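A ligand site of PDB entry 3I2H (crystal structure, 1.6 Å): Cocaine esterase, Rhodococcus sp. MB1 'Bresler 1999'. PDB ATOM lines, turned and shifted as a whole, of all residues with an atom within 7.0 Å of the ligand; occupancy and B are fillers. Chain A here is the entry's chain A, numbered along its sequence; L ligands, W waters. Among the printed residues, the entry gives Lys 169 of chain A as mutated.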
ATOM      1  N   PRO A  43       9.173  31.612 -11.666  1.00  0.00           N
ATOM      2  CA  PRO A  43       9.027  31.995 -13.079  1.00  0.00           C
ATOM      3  C   PRO A  43       7.605  32.450 -13.467  1.00  0.00           C
ATOM      4  O   PRO A  43       7.326  32.625 -14.664  1.00  0.00           O
ATOM      5  CB  PRO A  43       9.358  30.692 -13.809  1.00  0.00           C
ATOM      6  CG  PRO A  43       8.798  29.639 -12.895  1.00  0.00           C
ATOM      7  CD  PRO A  43       8.959  30.164 -11.474  1.00  0.00           C
ATOM      8  N   TYR A  44       6.732  32.631 -12.485  1.00  0.00           N
ATOM      9  CA  TYR A  44       5.323  32.933 -12.726  1.00  0.00           C
ATOM     10  C   TYR A  44       4.892  34.301 -12.178  1.00  0.00           C
ATOM     11  O   TYR A  44       3.720  34.483 -11.820  1.00  0.00           O
ATOM     12  CB  TYR A  44       4.425  31.826 -12.153  1.00  0.00           C
ATOM     13  CG  TYR A  44       4.849  30.405 -12.506  1.00  0.00           C
ATOM     14  CD1 TYR A  44       4.803  29.953 -13.818  1.00  0.00           C
ATOM     15  CD2 TYR A  44       5.278  29.528 -11.515  1.00  0.00           C
ATOM     16  CE1 TYR A  44       5.182  28.647 -14.146  1.00  0.00           C
ATOM     17  CE2 TYR A  44       5.657  28.225 -11.821  1.00  0.00           C
ATOM     18  CZ  TYR A  44       5.606  27.796 -13.139  1.00  0.00           C
ATOM     19  OH  TYR A  44       5.991  26.502 -13.437  1.00  0.00           O
ATOM     20  N   HIS A  87      15.736  25.956 -16.296  1.00  0.00           N
ATOM     21  CA  HIS A  87      16.727  25.176 -15.532  1.00  0.00           C
ATOM     22  C   HIS A  87      18.206  25.613 -15.608  1.00  0.00           C
ATOM     23  O   HIS A  87      18.923  25.541 -14.609  1.00  0.00           O
ATOM     24  CB  HIS A  87      16.647  23.673 -15.833  1.00  0.00           C
ATOM     25  CG  HIS A  87      15.249  23.127 -15.894  1.00  0.00           C
ATOM     26  ND1 HIS A  87      14.325  23.340 -14.900  1.00  0.00           N
ATOM     27  CD2 HIS A  87      14.650  22.345 -16.813  1.00  0.00           C
ATOM     28  CE1 HIS A  87      13.201  22.731 -15.209  1.00  0.00           C
ATOM     29  NE2 HIS A  87      13.373  22.113 -16.373  1.00  0.00           N
ATOM     30  N   VAL A 116       6.814  25.444  -4.202  1.00  0.00           N
ATOM     31  CA  VAL A 116       6.238  24.280  -4.861  1.00  0.00           C
ATOM     32  C   VAL A 116       6.619  24.239  -6.346  1.00  0.00           C
ATOM     33  O   VAL A 116       6.781  25.300  -6.974  1.00  0.00           O
ATOM     34  CB  VAL A 116       4.696  24.297  -4.675  1.00  0.00           C
ATOM     35  CG1 VAL A 116       4.046  25.499  -5.391  1.00  0.00           C
ATOM     36  CG2 VAL A 116       4.081  22.975  -5.111  1.00  0.00           C
ATOM     37  N   SER A 117       6.770  23.033  -6.887  1.00  0.00           N
ATOM     38  CA  SER A 117       6.951  22.837  -8.331  1.00  0.00           C
ATOM     39  C   SER A 117       8.265  23.492  -8.802  1.00  0.00           C
ATOM     40  O   SER A 117       9.332  23.107  -8.327  1.00  0.00           O
ATOM     41  CB  SER A 117       5.704  23.361  -9.081  1.00  0.00           C
ATOM     42  OG  SER A 117       5.586  22.800 -10.369  1.00  0.00           O
ATOM     43  N   TYR A 118       8.219  24.466  -9.709  1.00  0.00           N
ATOM     44  CA  TYR A 118       9.458  25.096 -10.194  1.00  0.00           C
ATOM     45  C   TYR A 118      10.128  25.842  -9.026  1.00  0.00           C
ATOM     46  O   TYR A 118      11.348  25.960  -8.982  1.00  0.00           O
ATOM     47  CB  TYR A 118       9.160  26.045 -11.355  1.00  0.00           C
ATOM     48  CG  TYR A 118      10.337  26.401 -12.244  1.00  0.00           C
ATOM     49  CD1 TYR A 118      11.256  27.397 -11.868  1.00  0.00           C
ATOM     50  CD2 TYR A 118      10.500  25.790 -13.490  1.00  0.00           C
ATOM     51  CE1 TYR A 118      12.317  27.759 -12.709  1.00  0.00           C
ATOM     52  CE2 TYR A 118      11.566  26.140 -14.334  1.00  0.00           C
ATOM     53  CZ  TYR A 118      12.464  27.123 -13.939  1.00  0.00           C
ATOM     54  OH  TYR A 118      13.498  27.463 -14.792  1.00  0.00           O
ATOM     55  N   LEU A 119       9.301  26.324  -8.098  1.00  0.00           N
ATOM     56  CA  LEU A 119       9.777  27.009  -6.885  1.00  0.00           C
ATOM     57  C   LEU A 119      10.387  26.010  -5.900  1.00  0.00           C
ATOM     58  O   LEU A 119      10.972  26.419  -4.892  1.00  0.00           O
ATOM     59  CB  LEU A 119       8.631  27.750  -6.210  1.00  0.00           C
ATOM     60  CG  LEU A 119       8.014  28.986  -6.883  1.00  0.00           C
ATOM     61  CD1 LEU A 119       7.491  28.697  -8.290  1.00  0.00           C
ATOM     62  CD2 LEU A 119       6.888  29.490  -6.014  1.00  0.00           C
ATOM     63  N   GLY A 120      10.199  24.720  -6.198  1.00  0.00           N
ATOM     64  CA  GLY A 120      10.822  23.617  -5.453  1.00  0.00           C
ATOM     65  C   GLY A 120      12.097  23.108  -6.113  1.00  0.00           C
ATOM     66  O   GLY A 120      13.119  22.909  -5.444  1.00  0.00           O
ATOM     67  N   VAL A 121      12.049  22.894  -7.420  1.00  0.00           N
ATOM     68  CA  VAL A 121      13.220  22.469  -8.183  1.00  0.00           C
ATOM     69  C   VAL A 121      14.387  23.441  -7.966  1.00  0.00           C
ATOM     70  O   VAL A 121      15.536  23.018  -7.776  1.00  0.00           O
ATOM     71  CB  VAL A 121      12.898  22.383  -9.703  1.00  0.00           C
ATOM     72  CG1 VAL A 121      14.157  22.164 -10.544  1.00  0.00           C
ATOM     73  CG2 VAL A 121      11.888  21.282  -9.972  1.00  0.00           C
ATOM     74  N   MET A 141       6.498  19.159  -4.071  1.00  0.00           N
ATOM     75  CA  MET A 141       6.113  18.633  -5.387  1.00  0.00           C
ATOM     76  C   MET A 141       7.216  18.959  -6.443  1.00  0.00           C
ATOM     77  O   MET A 141       6.929  19.595  -7.465  1.00  0.00           O
ATOM     78  CB  MET A 141       4.655  19.070  -5.762  1.00  0.00           C
ATOM     79  CG  MET A 141       3.579  18.486  -4.820  1.00  0.00           C
ATOM     80  SD  MET A 141       2.006  19.306  -5.026  1.00  0.00           S
ATOM     81  CE  MET A 141       0.884  17.913  -5.082  1.00  0.00           C
ATOM     82  N   LEU A 146      15.691  16.377 -13.656  1.00  0.00           N
ATOM     83  CA  LEU A 146      14.633  16.892 -14.528  1.00  0.00           C
ATOM     84  C   LEU A 146      14.247  15.924 -15.634  1.00  0.00           C
ATOM     85  O   LEU A 146      13.119  15.975 -16.138  1.00  0.00           O
ATOM     86  CB  LEU A 146      14.985  18.274 -15.086  1.00  0.00           C
ATOM     87  CG  LEU A 146      14.883  19.488 -14.152  1.00  0.00           C
ATOM     88  CD1 LEU A 146      13.550  19.554 -13.409  1.00  0.00           C
ATOM     89  CD2 LEU A 146      16.043  19.545 -13.177  1.00  0.00           C
ATOM     90  N   ALA A 149      11.842  13.476 -13.652  1.00  0.00           N
ATOM     91  CA  ALA A 149      10.589  14.220 -13.485  1.00  0.00           C
ATOM     92  C   ALA A 149      10.869  15.712 -13.625  1.00  0.00           C
ATOM     93  O   ALA A 149      11.783  16.219 -12.975  1.00  0.00           O
ATOM     94  CB  ALA A 149       9.945  13.930 -12.118  1.00  0.00           C
ATOM     95  N   PRO A 150      10.044  16.439 -14.386  1.00  0.00           N
ATOM     96  CA  PRO A 150       8.793  15.999 -15.011  1.00  0.00           C
ATOM     97  C   PRO A 150       8.852  15.683 -16.510  1.00  0.00           C
ATOM     98  O   PRO A 150       7.808  15.382 -17.093  1.00  0.00           O
ATOM     99  CB  PRO A 150       7.896  17.211 -14.810  1.00  0.00           C
ATOM    100  CG  PRO A 150       8.851  18.384 -15.024  1.00  0.00           C
ATOM    101  CD  PRO A 150      10.238  17.883 -14.591  1.00  0.00           C
ATOM    102  N   TRP A 151      10.030  15.751 -17.147  1.00  0.00           N
ATOM    103  CA  TRP A 151      10.048  15.754 -18.619  1.00  0.00           C
ATOM    104  C   TRP A 151      10.046  14.379 -19.291  1.00  0.00           C
ATOM    105  O   TRP A 151       9.353  14.183 -20.296  1.00  0.00           O
ATOM    106  CB  TRP A 151      11.157  16.664 -19.163  1.00  0.00           C
ATOM    107  CG  TRP A 151      11.121  18.055 -18.592  1.00  0.00           C
ATOM    108  CD1 TRP A 151      12.164  18.730 -18.028  1.00  0.00           C
ATOM    109  CD2 TRP A 151       9.969  18.916 -18.471  1.00  0.00           C
ATOM    110  NE1 TRP A 151      11.744  19.965 -17.590  1.00  0.00           N
ATOM    111  CE2 TRP A 151      10.410  20.107 -17.851  1.00  0.00           C
ATOM    112  CE3 TRP A 151       8.614  18.798 -18.848  1.00  0.00           C
ATOM    113  CZ2 TRP A 151       9.540  21.176 -17.584  1.00  0.00           C
ATOM    114  CZ3 TRP A 151       7.756  19.862 -18.575  1.00  0.00           C
ATOM    115  CH2 TRP A 151       8.218  21.036 -17.944  1.00  0.00           C
ATOM    116  N   ALA A 162       2.884  16.847 -20.160  1.00  0.00           N
ATOM    117  CA  ALA A 162       3.515  17.760 -19.214  1.00  0.00           C
ATOM    118  C   ALA A 162       4.320  18.810 -19.970  1.00  0.00           C
ATOM    119  O   ALA A 162       4.227  20.002 -19.681  1.00  0.00           O
ATOM    120  CB  ALA A 162       4.419  16.999 -18.271  1.00  0.00           C
ATOM    121  N   LEU A 163       5.106  18.352 -20.933  1.00  0.00           N
ATOM    122  CA  LEU A 163       5.946  19.245 -21.724  1.00  0.00           C
ATOM    123  C   LEU A 163       5.140  20.276 -22.495  1.00  0.00           C
ATOM    124  O   LEU A 163       5.430  21.481 -22.441  1.00  0.00           O
ATOM    125  CB  LEU A 163       6.826  18.450 -22.683  1.00  0.00           C
ATOM    126  CG  LEU A 163       7.714  19.327 -23.561  1.00  0.00           C
ATOM    127  CD1 LEU A 163       8.741  20.101 -22.701  1.00  0.00           C
ATOM    128  CD2 LEU A 163       8.400  18.499 -24.636  1.00  0.00           C
ATOM    129  N   GLY A 165       1.868  21.146 -22.240  1.00  0.00           N
ATOM    130  CA  GLY A 165       1.069  21.968 -21.335  1.00  0.00           C
ATOM    131  C   GLY A 165       1.887  23.042 -20.652  1.00  0.00           C
ATOM    132  O   GLY A 165       1.502  24.213 -20.634  1.00  0.00           O
ATOM    133  N   TRP A 166       3.026  22.649 -20.087  1.00  0.00           N
ATOM    134  CA  TRP A 166       3.849  23.627 -19.380  1.00  0.00           C
ATOM    135  C   TRP A 166       4.427  24.670 -20.324  1.00  0.00           C
ATOM    136  O   TRP A 166       4.452  25.862 -20.008  1.00  0.00           O
ATOM    137  CB  TRP A 166       4.974  22.957 -18.610  1.00  0.00           C
ATOM    138  CG  TRP A 166       5.686  23.911 -17.706  1.00  0.00           C
ATOM    139  CD1 TRP A 166       5.199  24.455 -16.546  1.00  0.00           C
ATOM    140  CD2 TRP A 166       7.001  24.454 -17.881  1.00  0.00           C
ATOM    141  NE1 TRP A 166       6.145  25.296 -15.986  1.00  0.00           N
ATOM    142  CE2 TRP A 166       7.259  25.298 -16.785  1.00  0.00           C
ATOM    143  CE3 TRP A 166       7.996  24.290 -18.870  1.00  0.00           C
ATOM    144  CZ2 TRP A 166       8.477  25.996 -16.639  1.00  0.00           C
ATOM    145  CZ3 TRP A 166       9.205  24.991 -18.720  1.00  0.00           C
ATOM    146  CH2 TRP A 166       9.427  25.819 -17.609  1.00  0.00           C
ATOM    147  N   LYS A 169       1.870  27.144 -21.001  1.00  0.00           N
ATOM    148  CA  LYS A 169       1.723  27.922 -19.751  1.00  0.00           C
ATOM    149  C   LYS A 169       2.786  29.041 -19.644  1.00  0.00           C
ATOM    150  O   LYS A 169       2.466  30.181 -19.341  1.00  0.00           O
ATOM    151  CB  LYS A 169       1.716  27.003 -18.484  1.00  0.00           C
ATOM    152  CG  LYS A 169       1.519  27.743 -17.150  1.00  0.00           C
ATOM    153  CD  LYS A 169       1.660  26.811 -15.988  1.00  0.00           C
ATOM    154  CE  LYS A 169       1.617  27.596 -14.694  1.00  0.00           C
ATOM    155  NZ  LYS A 169       1.141  26.743 -13.597  1.00  0.00           N
ATOM    156  N   PHE A 261       5.579  14.588  -9.915  1.00  0.00           N
ATOM    157  CA  PHE A 261       6.897  14.530  -9.294  1.00  0.00           C
ATOM    158  C   PHE A 261       7.059  13.487  -8.192  1.00  0.00           C
ATOM    159  O   PHE A 261       8.139  13.376  -7.606  1.00  0.00           O
ATOM    160  CB  PHE A 261       7.242  15.886  -8.679  1.00  0.00           C
ATOM    161  CG  PHE A 261       7.483  16.977  -9.686  1.00  0.00           C
ATOM    162  CD1 PHE A 261       6.450  17.796 -10.104  1.00  0.00           C
ATOM    163  CD2 PHE A 261       8.771  17.200 -10.174  1.00  0.00           C
ATOM    164  CE1 PHE A 261       6.692  18.829 -11.028  1.00  0.00           C
ATOM    165  CE2 PHE A 261       9.020  18.233 -11.079  1.00  0.00           C
ATOM    166  CZ  PHE A 261       7.984  19.030 -11.509  1.00  0.00           C
ATOM    167  N   HIS A 287      -0.976  17.568  -9.191  1.00  0.00           N
ATOM    168  CA  HIS A 287      -0.258  18.839  -9.213  1.00  0.00           C
ATOM    169  C   HIS A 287      -1.179  20.048  -9.143  1.00  0.00           C
ATOM    170  O   HIS A 287      -0.838  21.072  -8.536  1.00  0.00           O
ATOM    171  CB  HIS A 287       0.615  18.933 -10.459  1.00  0.00           C
ATOM    172  CG  HIS A 287       1.884  19.714 -10.253  1.00  0.00           C
ATOM    173  ND1 HIS A 287       2.876  19.286  -9.402  1.00  0.00           N
ATOM    174  CD2 HIS A 287       2.319  20.871 -10.805  1.00  0.00           C
ATOM    175  CE1 HIS A 287       3.872  20.160  -9.424  1.00  0.00           C
ATOM    176  NE2 HIS A 287       3.559  21.124 -10.263  1.00  0.00           N
ATOM    177  N   LEU A 407      -0.345  15.882 -15.527  1.00  0.00           N
ATOM    178  CA  LEU A 407      -0.053  17.245 -15.063  1.00  0.00           C
ATOM    179  C   LEU A 407      -0.993  18.301 -15.657  1.00  0.00           C
ATOM    180  O   LEU A 407      -1.614  19.050 -14.917  1.00  0.00           O
ATOM    181  CB  LEU A 407       1.424  17.599 -15.329  1.00  0.00           C
ATOM    182  CG  LEU A 407       2.445  16.932 -14.396  1.00  0.00           C
ATOM    183  CD1 LEU A 407       3.848  17.009 -14.931  1.00  0.00           C
ATOM    184  CD2 LEU A 407       2.409  17.559 -13.039  1.00  0.00           C
ATOM    185  N   PHE A 408      -1.098  18.311 -16.990  1.00  0.00           N
ATOM    186  CA  PHE A 408      -1.868  19.332 -17.722  1.00  0.00           C
ATOM    187  C   PHE A 408      -3.085  18.801 -18.476  1.00  0.00           C
ATOM    188  O   PHE A 408      -4.092  19.497 -18.610  1.00  0.00           O
ATOM    189  CB  PHE A 408      -0.960  20.118 -18.679  1.00  0.00           C
ATOM    190  CG  PHE A 408      -0.096  21.112 -17.976  1.00  0.00           C
ATOM    191  CD1 PHE A 408      -0.545  22.421 -17.782  1.00  0.00           C
ATOM    192  CD2 PHE A 408       1.141  20.749 -17.483  1.00  0.00           C
ATOM    193  CE1 PHE A 408       0.250  23.351 -17.120  1.00  0.00           C
ATOM    194  CE2 PHE A 408       1.933  21.661 -16.810  1.00  0.00           C
ATOM    195  CZ  PHE A 408       1.485  22.957 -16.628  1.00  0.00           C
HETATM  196  O1  LIG L   1       5.775  25.012 -11.327  1.00  0.00           O
HETATM  197  C1  LIG L   1       5.836  23.597 -11.605  1.00  0.00           C
HETATM  198  O2  LIG L   1       4.833  23.113 -12.585  1.00  0.00           O
HETATM  199  O3  LIG L   1       7.103  23.250 -12.175  1.00  0.00           O
HETATM  200  C2  LIG L   1       6.932  22.263 -13.176  1.00  0.00           C
HETATM  201  C3  LIG L   1       8.025  22.475 -14.224  1.00  0.00           C
HETATM  202  S1  LIG L   1       9.652  22.020 -13.584  1.00  0.00           S
HETATM  203  C4  LIG L   1       5.502  22.484 -13.674  1.00  0.00           C
HETATM  204  C5  LIG L   1       4.742  21.199 -13.972  1.00  0.00           C
HETATM  205  S2  LIG L   1       5.390  20.288 -15.395  1.00  0.00           S
HETATM  206  O   HOH W   1       2.658  24.489 -13.438  1.00  0.00           O
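OG of Ser 117 is bonded to C1 of the ligand.
The side-chain hydroxyl of Tyr 44 is in hydrogen-bond range of an oxygen (O1) of the ligand, at 2.6 Å.
The backbone NH (N) of Tyr 118 lies within hydrogen-bond range of an oxygen (O3) of the ligand (3.0 Å).
An oxygen (O2) of the ligand lies within hydrogen-bond range of a ring nitrogen (NE2) of His 287 (3.3 Å).
His 87 touches the ligand (CE1 to S1, 3.97 Å).
Pro 150 touches the ligand.
Trp 151 touches the ligand.
CD1 of Trp 166 touches C4 of the ligand, 3.5 Å away.
CZ of Phe 261 touches C2 of the ligand, at 3.8 Å.
Leu 407 touches the ligand.
CE2 of Phe 408 touches S2 of the ligand, 3.98 Å away.
Within 4 Å of the ligand: Tyr 44, His 87, Ser 117, Tyr 118, Pro 150, Trp 151, Trp 166, Phe 261, His 287, Leu 407 and Phe 408.
OG of Ser 117 sits at hydrogen-bond distance from NE2 of His 287, at 2.6 Å.
The backbone NH (N) of Ser 117 sits close to the backbone carbonyl oxygen (O) of Met 141.
The indole nitrogen (NE1) of Trp 166 lies within hydrogen-bond range of the side-chain hydroxyl (OH) of Tyr 44 (2.8 Å).
The backbone NH (N) of His 87 is in hydrogen-bond range of the side-chain hydroxyl (OH) of Tyr 118 (3.1 Å).
The indole nitrogen (NE1) of Trp 151 sits at hydrogen-bond distance from a ring nitrogen (NE2) of His 87 (3.0 Å).
O of Leu 146 is in hydrogen-bond range of N of Trp 151, at 3.3 Å.
Water W1 lies within hydrogen-bond range of O2 of the ligand (2.7 Å) and NZ of Lys 169 (2.7 Å).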
